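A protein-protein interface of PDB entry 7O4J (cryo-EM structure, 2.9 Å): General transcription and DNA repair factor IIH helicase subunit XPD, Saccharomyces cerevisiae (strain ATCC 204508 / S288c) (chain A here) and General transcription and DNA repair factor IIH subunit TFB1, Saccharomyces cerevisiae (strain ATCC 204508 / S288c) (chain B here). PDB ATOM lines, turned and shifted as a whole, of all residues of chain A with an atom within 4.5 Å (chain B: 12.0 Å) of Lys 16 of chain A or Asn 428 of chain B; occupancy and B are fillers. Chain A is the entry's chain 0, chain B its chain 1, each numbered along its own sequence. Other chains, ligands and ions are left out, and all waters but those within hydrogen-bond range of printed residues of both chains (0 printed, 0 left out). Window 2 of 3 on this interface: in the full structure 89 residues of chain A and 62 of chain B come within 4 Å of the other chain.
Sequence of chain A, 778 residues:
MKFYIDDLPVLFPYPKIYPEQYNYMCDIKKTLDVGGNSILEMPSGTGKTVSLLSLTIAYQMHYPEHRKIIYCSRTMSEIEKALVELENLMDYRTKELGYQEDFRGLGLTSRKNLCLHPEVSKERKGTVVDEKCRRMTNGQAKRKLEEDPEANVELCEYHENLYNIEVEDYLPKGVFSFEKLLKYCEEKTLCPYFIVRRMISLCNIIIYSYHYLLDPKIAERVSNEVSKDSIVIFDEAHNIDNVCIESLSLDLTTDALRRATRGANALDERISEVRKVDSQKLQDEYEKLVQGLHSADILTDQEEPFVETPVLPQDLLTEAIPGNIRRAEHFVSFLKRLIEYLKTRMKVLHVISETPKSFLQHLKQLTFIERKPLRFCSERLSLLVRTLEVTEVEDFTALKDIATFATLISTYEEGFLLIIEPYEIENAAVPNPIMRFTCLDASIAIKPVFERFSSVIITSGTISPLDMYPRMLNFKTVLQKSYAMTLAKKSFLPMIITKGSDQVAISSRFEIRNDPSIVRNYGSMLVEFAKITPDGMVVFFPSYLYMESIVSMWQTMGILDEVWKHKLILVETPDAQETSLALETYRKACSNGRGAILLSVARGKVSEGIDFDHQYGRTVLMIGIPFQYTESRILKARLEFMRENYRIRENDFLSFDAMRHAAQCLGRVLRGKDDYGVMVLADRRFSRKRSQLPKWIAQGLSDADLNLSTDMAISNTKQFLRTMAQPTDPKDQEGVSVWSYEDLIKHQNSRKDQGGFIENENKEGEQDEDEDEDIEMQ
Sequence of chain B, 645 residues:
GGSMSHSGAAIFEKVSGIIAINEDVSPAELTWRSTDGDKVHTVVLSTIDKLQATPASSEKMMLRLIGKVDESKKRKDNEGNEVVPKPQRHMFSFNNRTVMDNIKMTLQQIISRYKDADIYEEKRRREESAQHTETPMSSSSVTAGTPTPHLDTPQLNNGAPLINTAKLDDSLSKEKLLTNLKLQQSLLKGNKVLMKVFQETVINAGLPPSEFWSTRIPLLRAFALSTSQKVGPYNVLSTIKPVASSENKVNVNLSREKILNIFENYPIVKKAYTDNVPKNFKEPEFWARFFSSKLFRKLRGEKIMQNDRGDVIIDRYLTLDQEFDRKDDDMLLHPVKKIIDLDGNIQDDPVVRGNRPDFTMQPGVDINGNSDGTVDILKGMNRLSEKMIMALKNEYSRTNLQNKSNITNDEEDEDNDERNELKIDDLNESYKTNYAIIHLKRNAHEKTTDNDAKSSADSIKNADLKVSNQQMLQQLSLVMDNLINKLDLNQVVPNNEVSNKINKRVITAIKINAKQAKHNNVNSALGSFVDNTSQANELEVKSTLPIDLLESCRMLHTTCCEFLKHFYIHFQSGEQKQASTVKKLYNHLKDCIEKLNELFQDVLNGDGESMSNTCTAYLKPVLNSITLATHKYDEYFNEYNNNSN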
ATOM      1  N   MET A   1     -21.632   8.398  23.903  1.00  0.00           N
ATOM      2  CA  MET A   1     -22.617   8.603  25.001  1.00  0.00           C
ATOM      3  C   MET A   1     -22.639  10.061  25.444  1.00  0.00           C
ATOM      4  O   MET A   1     -21.787  10.854  25.046  1.00  0.00           O
ATOM      5  CB  MET A   1     -22.290   7.694  26.189  1.00  0.00           C
ATOM      6  CG  MET A   1     -21.004   8.051  26.925  1.00  0.00           C
ATOM      7  SD  MET A   1     -20.801   7.124  28.458  1.00  0.00           S
ATOM      8  CE  MET A   1     -20.641   5.456  27.829  1.00  0.00           C
ATOM      9  N   PHE A  12     -19.299  12.055  25.011  1.00  0.00           N
ATOM     10  CA  PHE A  12     -18.228  11.162  24.582  1.00  0.00           C
ATOM     11  C   PHE A  12     -18.525  10.646  23.178  1.00  0.00           C
ATOM     12  O   PHE A  12     -19.677  10.303  22.886  1.00  0.00           O
ATOM     13  CB  PHE A  12     -18.083   9.991  25.544  1.00  0.00           C
ATOM     14  CG  PHE A  12     -16.700   9.405  25.588  1.00  0.00           C
ATOM     15  CD1 PHE A  12     -15.605  10.194  25.897  1.00  0.00           C
ATOM     16  CD2 PHE A  12     -16.497   8.063  25.320  1.00  0.00           C
ATOM     17  CE1 PHE A  12     -14.337   9.656  25.934  1.00  0.00           C
ATOM     18  CE2 PHE A  12     -15.230   7.520  25.357  1.00  0.00           C
ATOM     19  CZ  PHE A  12     -14.148   8.318  25.665  1.00  0.00           C
ATOM     20  N   TYR A  14     -18.039   7.916  21.812  1.00  0.00           N
ATOM     21  CA  TYR A  14     -18.159   6.469  21.760  1.00  0.00           C
ATOM     22  C   TYR A  14     -19.327   6.015  22.621  1.00  0.00           C
ATOM     23  O   TYR A  14     -19.658   6.665  23.617  1.00  0.00           O
ATOM     24  CB  TYR A  14     -16.875   5.788  22.250  1.00  0.00           C
ATOM     25  CG  TYR A  14     -15.672   6.038  21.370  1.00  0.00           C
ATOM     26  CD1 TYR A  14     -15.481   5.317  20.200  1.00  0.00           C
ATOM     27  CD2 TYR A  14     -14.726   6.992  21.712  1.00  0.00           C
ATOM     28  CE1 TYR A  14     -14.384   5.542  19.394  1.00  0.00           C
ATOM     29  CE2 TYR A  14     -13.625   7.225  20.913  1.00  0.00           C
ATOM     30  CZ  TYR A  14     -13.458   6.497  19.756  1.00  0.00           C
ATOM     31  OH  TYR A  14     -12.362   6.726  18.957  1.00  0.00           O
ATOM     32  N   PRO A  15     -19.975   4.902  22.262  1.00  0.00           N
ATOM     33  CA  PRO A  15     -21.049   4.378  23.120  1.00  0.00           C
ATOM     34  C   PRO A  15     -20.540   3.749  24.403  1.00  0.00           C
ATOM     35  O   PRO A  15     -21.304   3.651  25.370  1.00  0.00           O
ATOM     36  CB  PRO A  15     -21.737   3.342  22.225  1.00  0.00           C
ATOM     37  CG  PRO A  15     -20.668   2.884  21.301  1.00  0.00           C
ATOM     38  CD  PRO A  15     -19.770   4.067  21.065  1.00  0.00           C
ATOM     39  N   LYS A  16     -19.280   3.325  24.441  1.00  0.00           N
ATOM     40  CA  LYS A  16     -18.665   2.738  25.620  1.00  0.00           C
ATOM     41  C   LYS A  16     -17.567   3.658  26.138  1.00  0.00           C
ATOM     42  O   LYS A  16     -17.095   4.555  25.434  1.00  0.00           O
ATOM     43  CB  LYS A  16     -18.087   1.356  25.303  1.00  0.00           C
ATOM     44  CG  LYS A  16     -19.131   0.323  24.910  1.00  0.00           C
ATOM     45  CD  LYS A  16     -18.486  -0.920  24.317  1.00  0.00           C
ATOM     46  CE  LYS A  16     -19.527  -1.936  23.877  1.00  0.00           C
ATOM     47  NZ  LYS A  16     -20.390  -2.383  25.006  1.00  0.00           N
ATOM     48  N   ILE A  17     -17.166   3.429  27.387  1.00  0.00           N
ATOM     49  CA  ILE A  17     -16.145   4.247  28.028  1.00  0.00           C
ATOM     50  C   ILE A  17     -15.403   3.392  29.043  1.00  0.00           C
ATOM     51  O   ILE A  17     -15.985   2.518  29.690  1.00  0.00           O
ATOM     52  CB  ILE A  17     -16.762   5.496  28.699  1.00  0.00           C
ATOM     53  CG1 ILE A  17     -15.676   6.532  28.991  1.00  0.00           C
ATOM     54  CG2 ILE A  17     -17.493   5.111  29.974  1.00  0.00           C
ATOM     55  CD1 ILE A  17     -16.209   7.824  29.564  1.00  0.00           C
ATOM     56  N   VAL A 738     -14.982  -2.246  30.666  1.00  0.00           N
ATOM     57  CA  VAL A 738     -15.663  -1.398  29.699  1.00  0.00           C
ATOM     58  C   VAL A 738     -17.045  -1.079  30.245  1.00  0.00           C
ATOM     59  O   VAL A 738     -17.757  -1.960  30.738  1.00  0.00           O
ATOM     60  CB  VAL A 738     -15.763  -2.064  28.311  1.00  0.00           C
ATOM     61  CG1 VAL A 738     -16.423  -1.123  27.319  1.00  0.00           C
ATOM     62  CG2 VAL A 738     -14.387  -2.487  27.823  1.00  0.00           C
ATOM     63  N   TRP A 739     -17.426   0.192  30.153  1.00  0.00           N
ATOM     64  CA  TRP A 739     -18.662   0.686  30.739  1.00  0.00           C
ATOM     65  C   TRP A 739     -19.614   1.156  29.650  1.00  0.00           C
ATOM     66  O   TRP A 739     -19.220   1.893  28.741  1.00  0.00           O
ATOM     67  CB  TRP A 739     -18.395   1.848  31.702  1.00  0.00           C
ATOM     68  CG  TRP A 739     -17.850   1.439  33.034  1.00  0.00           C
ATOM     69  CD1 TRP A 739     -17.643   0.170  33.485  1.00  0.00           C
ATOM     70  CD2 TRP A 739     -17.437   2.312  34.090  1.00  0.00           C
ATOM     71  NE1 TRP A 739     -17.130   0.199  34.758  1.00  0.00           N
ATOM     72  CE2 TRP A 739     -16.994   1.503  35.152  1.00  0.00           C
ATOM     73  CE3 TRP A 739     -17.401   3.700  34.239  1.00  0.00           C
ATOM     74  CZ2 TRP A 739     -16.519   2.036  36.347  1.00  0.00           C
ATOM     75  CZ3 TRP A 739     -16.931   4.227  35.425  1.00  0.00           C
ATOM     76  CH2 TRP A 739     -16.496   3.397  36.463  1.00  0.00           C
ATOM     77  N   GLU B 418      -6.910   7.800   7.314  1.00  0.00           N
ATOM     78  CA  GLU B 418      -6.233   8.069   8.579  1.00  0.00           C
ATOM     79  C   GLU B 418      -7.220   8.070   9.741  1.00  0.00           C
ATOM     80  O   GLU B 418      -6.906   7.595  10.838  1.00  0.00           O
ATOM     81  CB  GLU B 418      -5.477   9.400   8.503  1.00  0.00           C
ATOM     82  CG  GLU B 418      -6.348  10.657   8.533  1.00  0.00           C
ATOM     83  CD  GLU B 418      -7.243  10.791   7.318  1.00  0.00           C
ATOM     84  OE1 GLU B 418      -8.326  11.399   7.440  1.00  0.00           O
ATOM     85  OE2 GLU B 418      -6.863  10.287   6.239  1.00  0.00           O
ATOM     86  N   ARG B 419      -8.426   8.597   9.517  1.00  0.00           N
ATOM     87  CA  ARG B 419      -9.405   8.694  10.594  1.00  0.00           C
ATOM     88  C   ARG B 419      -9.730   7.322  11.170  1.00  0.00           C
ATOM     89  O   ARG B 419      -9.830   7.154  12.390  1.00  0.00           O
ATOM     90  CB  ARG B 419     -10.677   9.375  10.085  1.00  0.00           C
ATOM     91  CG  ARG B 419     -10.520  10.871   9.825  1.00  0.00           C
ATOM     92  CD  ARG B 419     -11.833  11.638   9.980  1.00  0.00           C
ATOM     93  NE  ARG B 419     -12.560  11.283  11.196  1.00  0.00           N
ATOM     94  CZ  ARG B 419     -13.852  11.527  11.398  1.00  0.00           C
ATOM     95  NH1 ARG B 419     -14.423  11.163  12.537  1.00  0.00           N
ATOM     96  NH2 ARG B 419     -14.576  12.134  10.465  1.00  0.00           N
ATOM     97  N   ASN B 420      -9.898   6.322  10.302  1.00  0.00           N
ATOM     98  CA  ASN B 420     -10.272   4.993  10.775  1.00  0.00           C
ATOM     99  C   ASN B 420      -9.202   4.409  11.689  1.00  0.00           C
ATOM    100  O   ASN B 420      -9.518   3.813  12.725  1.00  0.00           O
ATOM    101  CB  ASN B 420     -10.523   4.064   9.586  1.00  0.00           C
ATOM    102  CG  ASN B 420     -11.378   4.707   8.511  1.00  0.00           C
ATOM    103  OD1 ASN B 420     -10.872   5.143   7.478  1.00  0.00           O
ATOM    104  ND2 ASN B 420     -12.681   4.769   8.751  1.00  0.00           N
ATOM    105  N   GLU B 421      -7.928   4.569  11.324  1.00  0.00           N
ATOM    106  CA  GLU B 421      -6.854   3.987  12.123  1.00  0.00           C
ATOM    107  C   GLU B 421      -6.752   4.642  13.495  1.00  0.00           C
ATOM    108  O   GLU B 421      -6.418   3.967  14.477  1.00  0.00           O
ATOM    109  CB  GLU B 421      -5.525   4.109  11.376  1.00  0.00           C
ATOM    110  CG  GLU B 421      -4.310   3.601  12.148  1.00  0.00           C
ATOM    111  CD  GLU B 421      -4.431   2.145  12.561  1.00  0.00           C
ATOM    112  OE1 GLU B 421      -5.355   1.457  12.079  1.00  0.00           O
ATOM    113  OE2 GLU B 421      -3.599   1.688  13.372  1.00  0.00           O
ATOM    114  N   LEU B 422      -7.030   5.943  13.587  1.00  0.00           N
ATOM    115  CA  LEU B 422      -6.916   6.650  14.857  1.00  0.00           C
ATOM    116  C   LEU B 422      -8.054   6.337  15.817  1.00  0.00           C
ATOM    117  O   LEU B 422      -7.906   6.564  17.023  1.00  0.00           O
ATOM    118  CB  LEU B 422      -6.862   8.161  14.612  1.00  0.00           C
ATOM    119  CG  LEU B 422      -5.482   8.788  14.392  1.00  0.00           C
ATOM    120  CD1 LEU B 422      -4.603   8.599  15.617  1.00  0.00           C
ATOM    121  CD2 LEU B 422      -4.805   8.212  13.157  1.00  0.00           C
ATOM    122  N   LYS B 423      -9.177   5.827  15.322  1.00  0.00           N
ATOM    123  CA  LYS B 423     -10.324   5.557  16.176  1.00  0.00           C
ATOM    124  C   LYS B 423     -10.075   4.334  17.050  1.00  0.00           C
ATOM    125  O   LYS B 423      -9.370   3.397  16.664  1.00  0.00           O
ATOM    126  CB  LYS B 423     -11.582   5.347  15.333  1.00  0.00           C
ATOM    127  CG  LYS B 423     -12.125   6.625  14.716  1.00  0.00           C
ATOM    128  CD  LYS B 423     -13.295   6.346  13.784  1.00  0.00           C
ATOM    129  CE  LYS B 423     -14.568   6.038  14.556  1.00  0.00           C
ATOM    130  NZ  LYS B 423     -15.052   7.212  15.334  1.00  0.00           N
ATOM    131  N   ILE B 424     -10.668   4.352  18.242  1.00  0.00           N
ATOM    132  CA  ILE B 424     -10.535   3.262  19.204  1.00  0.00           C
ATOM    133  C   ILE B 424     -11.659   2.271  18.917  1.00  0.00           C
ATOM    134  O   ILE B 424     -12.822   2.517  19.240  1.00  0.00           O
ATOM    135  CB  ILE B 424     -10.580   3.769  20.646  1.00  0.00           C
ATOM    136  CG1 ILE B 424      -9.632   4.958  20.827  1.00  0.00           C
ATOM    137  CG2 ILE B 424     -10.216   2.651  21.613  1.00  0.00           C
ATOM    138  CD1 ILE B 424      -9.693   5.587  22.201  1.00  0.00           C
ATOM    139  N   ASP B 425     -11.306   1.138  18.307  1.00  0.00           N
ATOM    140  CA  ASP B 425     -12.314   0.151  17.935  1.00  0.00           C
ATOM    141  C   ASP B 425     -12.961  -0.489  19.157  1.00  0.00           C
ATOM    142  O   ASP B 425     -14.166  -0.768  19.142  1.00  0.00           O
ATOM    143  CB  ASP B 425     -11.689  -0.926  17.049  1.00  0.00           C
ATOM    144  CG  ASP B 425     -11.689  -0.548  15.581  1.00  0.00           C
ATOM    145  OD1 ASP B 425     -12.719  -0.033  15.097  1.00  0.00           O
ATOM    146  OD2 ASP B 425     -10.657  -0.764  14.912  1.00  0.00           O
ATOM    147  N   ASP B 426     -12.189  -0.731  20.217  1.00  0.00           N
ATOM    148  CA  ASP B 426     -12.711  -1.456  21.369  1.00  0.00           C
ATOM    149  C   ASP B 426     -13.869  -0.734  22.041  1.00  0.00           C
ATOM    150  O   ASP B 426     -14.670  -1.378  22.726  1.00  0.00           O
ATOM    151  CB  ASP B 426     -11.595  -1.694  22.387  1.00  0.00           C
ATOM    152  CG  ASP B 426     -12.037  -2.571  23.541  1.00  0.00           C
ATOM    153  OD1 ASP B 426     -12.769  -3.553  23.296  1.00  0.00           O
ATOM    154  OD2 ASP B 426     -11.655  -2.279  24.693  1.00  0.00           O
ATOM    155  N   LEU B 427     -13.980   0.580  21.867  1.00  0.00           N
ATOM    156  CA  LEU B 427     -15.040   1.355  22.496  1.00  0.00           C
ATOM    157  C   LEU B 427     -16.294   1.454  21.637  1.00  0.00           C
ATOM    158  O   LEU B 427     -17.266   2.086  22.062  1.00  0.00           O
ATOM    159  CB  LEU B 427     -14.535   2.764  22.824  1.00  0.00           C
ATOM    160  CG  LEU B 427     -13.493   2.856  23.940  1.00  0.00           C
ATOM    161  CD1 LEU B 427     -12.896   4.251  23.998  1.00  0.00           C
ATOM    162  CD2 LEU B 427     -14.103   2.479  25.281  1.00  0.00           C
ATOM    163  N   ASN B 428     -16.300   0.851  20.454  1.00  0.00           N
ATOM    164  CA  ASN B 428     -17.456   0.893  19.572  1.00  0.00           C
ATOM    165  C   ASN B 428     -18.382  -0.290  19.846  1.00  0.00           C
ATOM    166  O   ASN B 428     -18.030  -1.246  20.540  1.00  0.00           O
ATOM    167  CB  ASN B 428     -17.011   0.896  18.110  1.00  0.00           C
ATOM    168  CG  ASN B 428     -16.811   2.296  17.563  1.00  0.00           C
ATOM    169  OD1 ASN B 428     -17.556   3.218  17.898  1.00  0.00           O
ATOM    170  ND2 ASN B 428     -15.802   2.463  16.718  1.00  0.00           N
ATOM    171  N   GLU B 429     -19.587  -0.211  19.286  1.00  0.00           N
ATOM    172  CA  GLU B 429     -20.577  -1.260  19.494  1.00  0.00           C
ATOM    173  C   GLU B 429     -20.081  -2.583  18.925  1.00  0.00           C
ATOM    174  O   GLU B 429     -19.452  -2.628  17.864  1.00  0.00           O
ATOM    175  CB  GLU B 429     -21.904  -0.867  18.843  1.00  0.00           C
ATOM    176  CG  GLU B 429     -23.035  -1.858  19.081  1.00  0.00           C
ATOM    177  CD  GLU B 429     -23.384  -2.005  20.548  1.00  0.00           C
ATOM    178  OE1 GLU B 429     -23.093  -1.074  21.327  1.00  0.00           O
ATOM    179  OE2 GLU B 429     -23.950  -3.054  20.924  1.00  0.00           O
ATOM    180  N   SER B 430     -20.372  -3.666  19.639  1.00  0.00           N
ATOM    181  CA  SER B 430     -19.948  -4.989  19.202  1.00  0.00           C
ATOM    182  C   SER B 430     -20.676  -5.389  17.925  1.00  0.00           C
ATOM    183  O   SER B 430     -21.832  -5.017  17.705  1.00  0.00           O
ATOM    184  CB  SER B 430     -20.212  -6.019  20.300  1.00  0.00           C
ATOM    185  OG  SER B 430     -19.801  -5.531  21.565  1.00  0.00           O
ATOM    186  N   TYR B 431     -19.989  -6.155  17.080  1.00  0.00           N
ATOM    187  CA  TYR B 431     -20.586  -6.611  15.833  1.00  0.00           C
ATOM    188  C   TYR B 431     -21.817  -7.462  16.113  1.00  0.00           C
ATOM    189  O   TYR B 431     -21.829  -8.286  17.032  1.00  0.00           O
ATOM    190  CB  TYR B 431     -19.565  -7.410  15.022  1.00  0.00           C
ATOM    191  CG  TYR B 431     -20.161  -8.151  13.846  1.00  0.00           C
ATOM    192  CD1 TYR B 431     -20.369  -7.510  12.633  1.00  0.00           C
ATOM    193  CD2 TYR B 431     -20.508  -9.490  13.947  1.00  0.00           C
ATOM    194  CE1 TYR B 431     -20.912  -8.182  11.555  1.00  0.00           C
ATOM    195  CE2 TYR B 431     -21.051 -10.171  12.875  1.00  0.00           C
ATOM    196  CZ  TYR B 431     -21.251  -9.512  11.681  1.00  0.00           C
ATOM    197  OH  TYR B 431     -21.791 -10.184  10.609  1.00  0.00           O
ATOM    198  N   LYS B 432     -22.860  -7.256  15.312  1.00  0.00           N
ATOM    199  CA  LYS B 432     -24.122  -7.971  15.449  1.00  0.00           C
ATOM    200  C   LYS B 432     -24.370  -8.797  14.197  1.00  0.00           C
ATOM    201  O   LYS B 432     -24.289  -8.277  13.079  1.00  0.00           O
ATOM    202  CB  LYS B 432     -25.281  -6.999  15.682  1.00  0.00           C
ATOM    203  CG  LYS B 432     -26.593  -7.675  16.044  1.00  0.00           C
ATOM    204  CD  LYS B 432     -27.702  -6.659  16.283  1.00  0.00           C
ATOM    205  CE  LYS B 432     -27.546  -5.953  17.621  1.00  0.00           C
ATOM    206  NZ  LYS B 432     -27.667  -6.889  18.774  1.00  0.00           N
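Hydrophobic or aromatic side chains of chain B that line the printed part of chain A: Ile 424 and Leu 427. Hydrophobic or aromatic side chains of chain A within 4 Å of the printed part of chain B: Tyr 14 and Pro 15. Along chain A the printed residues that touch a printed residue of chain B span positions 14 to 17. Among the printed residues, 10 pairs touch across the chains.
Tyr 14 of chain A touches Lys 423 of chain B. Tyr 14 of chain A touches Leu 427 of chain B. Asn 428 of chain B touches Tyr 14 of chain A (OD1 to CD1, 3.7 Å). Leu 427 of chain B touches Pro 15 of chain A (O to CD, 3.3 Å). CD of Pro 15 of chain A touches OD1 of Asn 428 of chain B, 3.96 Å away. Pro 15 of chain A touches Glu 429 of chain B (CG to N, 3.8 Å). Lys 16 of chain A touches Asn 428 of chain B (CE to O, 3.7 Å). N of Ile 17 of chain A touches CD2 of Leu 427 of chain B, at 3.8 Å.
Lys 16 of chain A touches just these residues of chain B: Leu 427 and Asn 428. No residue of chain B comes within 4 Å of Met 1 of chain A. No residue of chain B comes within 4 Å of Phe 12 of chain A. Tyr 14 of chain A touches just these residues of chain B: Lys 423 (3.6 Å), Ile 424 (3.0 Å), Leu 427 (3.7 Å) and Asn 428 (3.7 Å). Of chain B, only Leu 427 (3.3 Å), Asn 428 (3.96 Å) and Glu 429 (3.8 Å) come within 4 Å of Pro 15 of chain A. No residue of chain B comes within 4 Å of Val 738 of chain A. Of the printed residues of chain A, Glu 429 of chain B touches Pro 15 (3.8 Å). Printed residues of chain A within 4 Å of Ile 424 of chain B: Tyr 14. The nearest printed residue of chain A that does not touch Asn 428 of chain B is Val 738 of chain A (7.0 Å). The nearest printed residue of chain A that does not touch Lys 423 of chain B is Pro 15 of chain A (8.1 Å).
N of Met 1 of chain A lies within hydrogen-bond range of O of Tyr 14 of chain A (2.6 Å). O of Ile 17 of chain A is in hydrogen-bond range of N of Trp 739 of chain A.
The side-chain hydroxyl of Tyr 14 of chain A lies within hydrogen-bond range of the backbone NH of Ile 424 of chain B (3.0 Å). The backbone NH of Lys 16 of chain A sits at hydrogen-bond distance from the backbone carbonyl oxygen of Leu 427 of chain B, at 3.4 Å.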
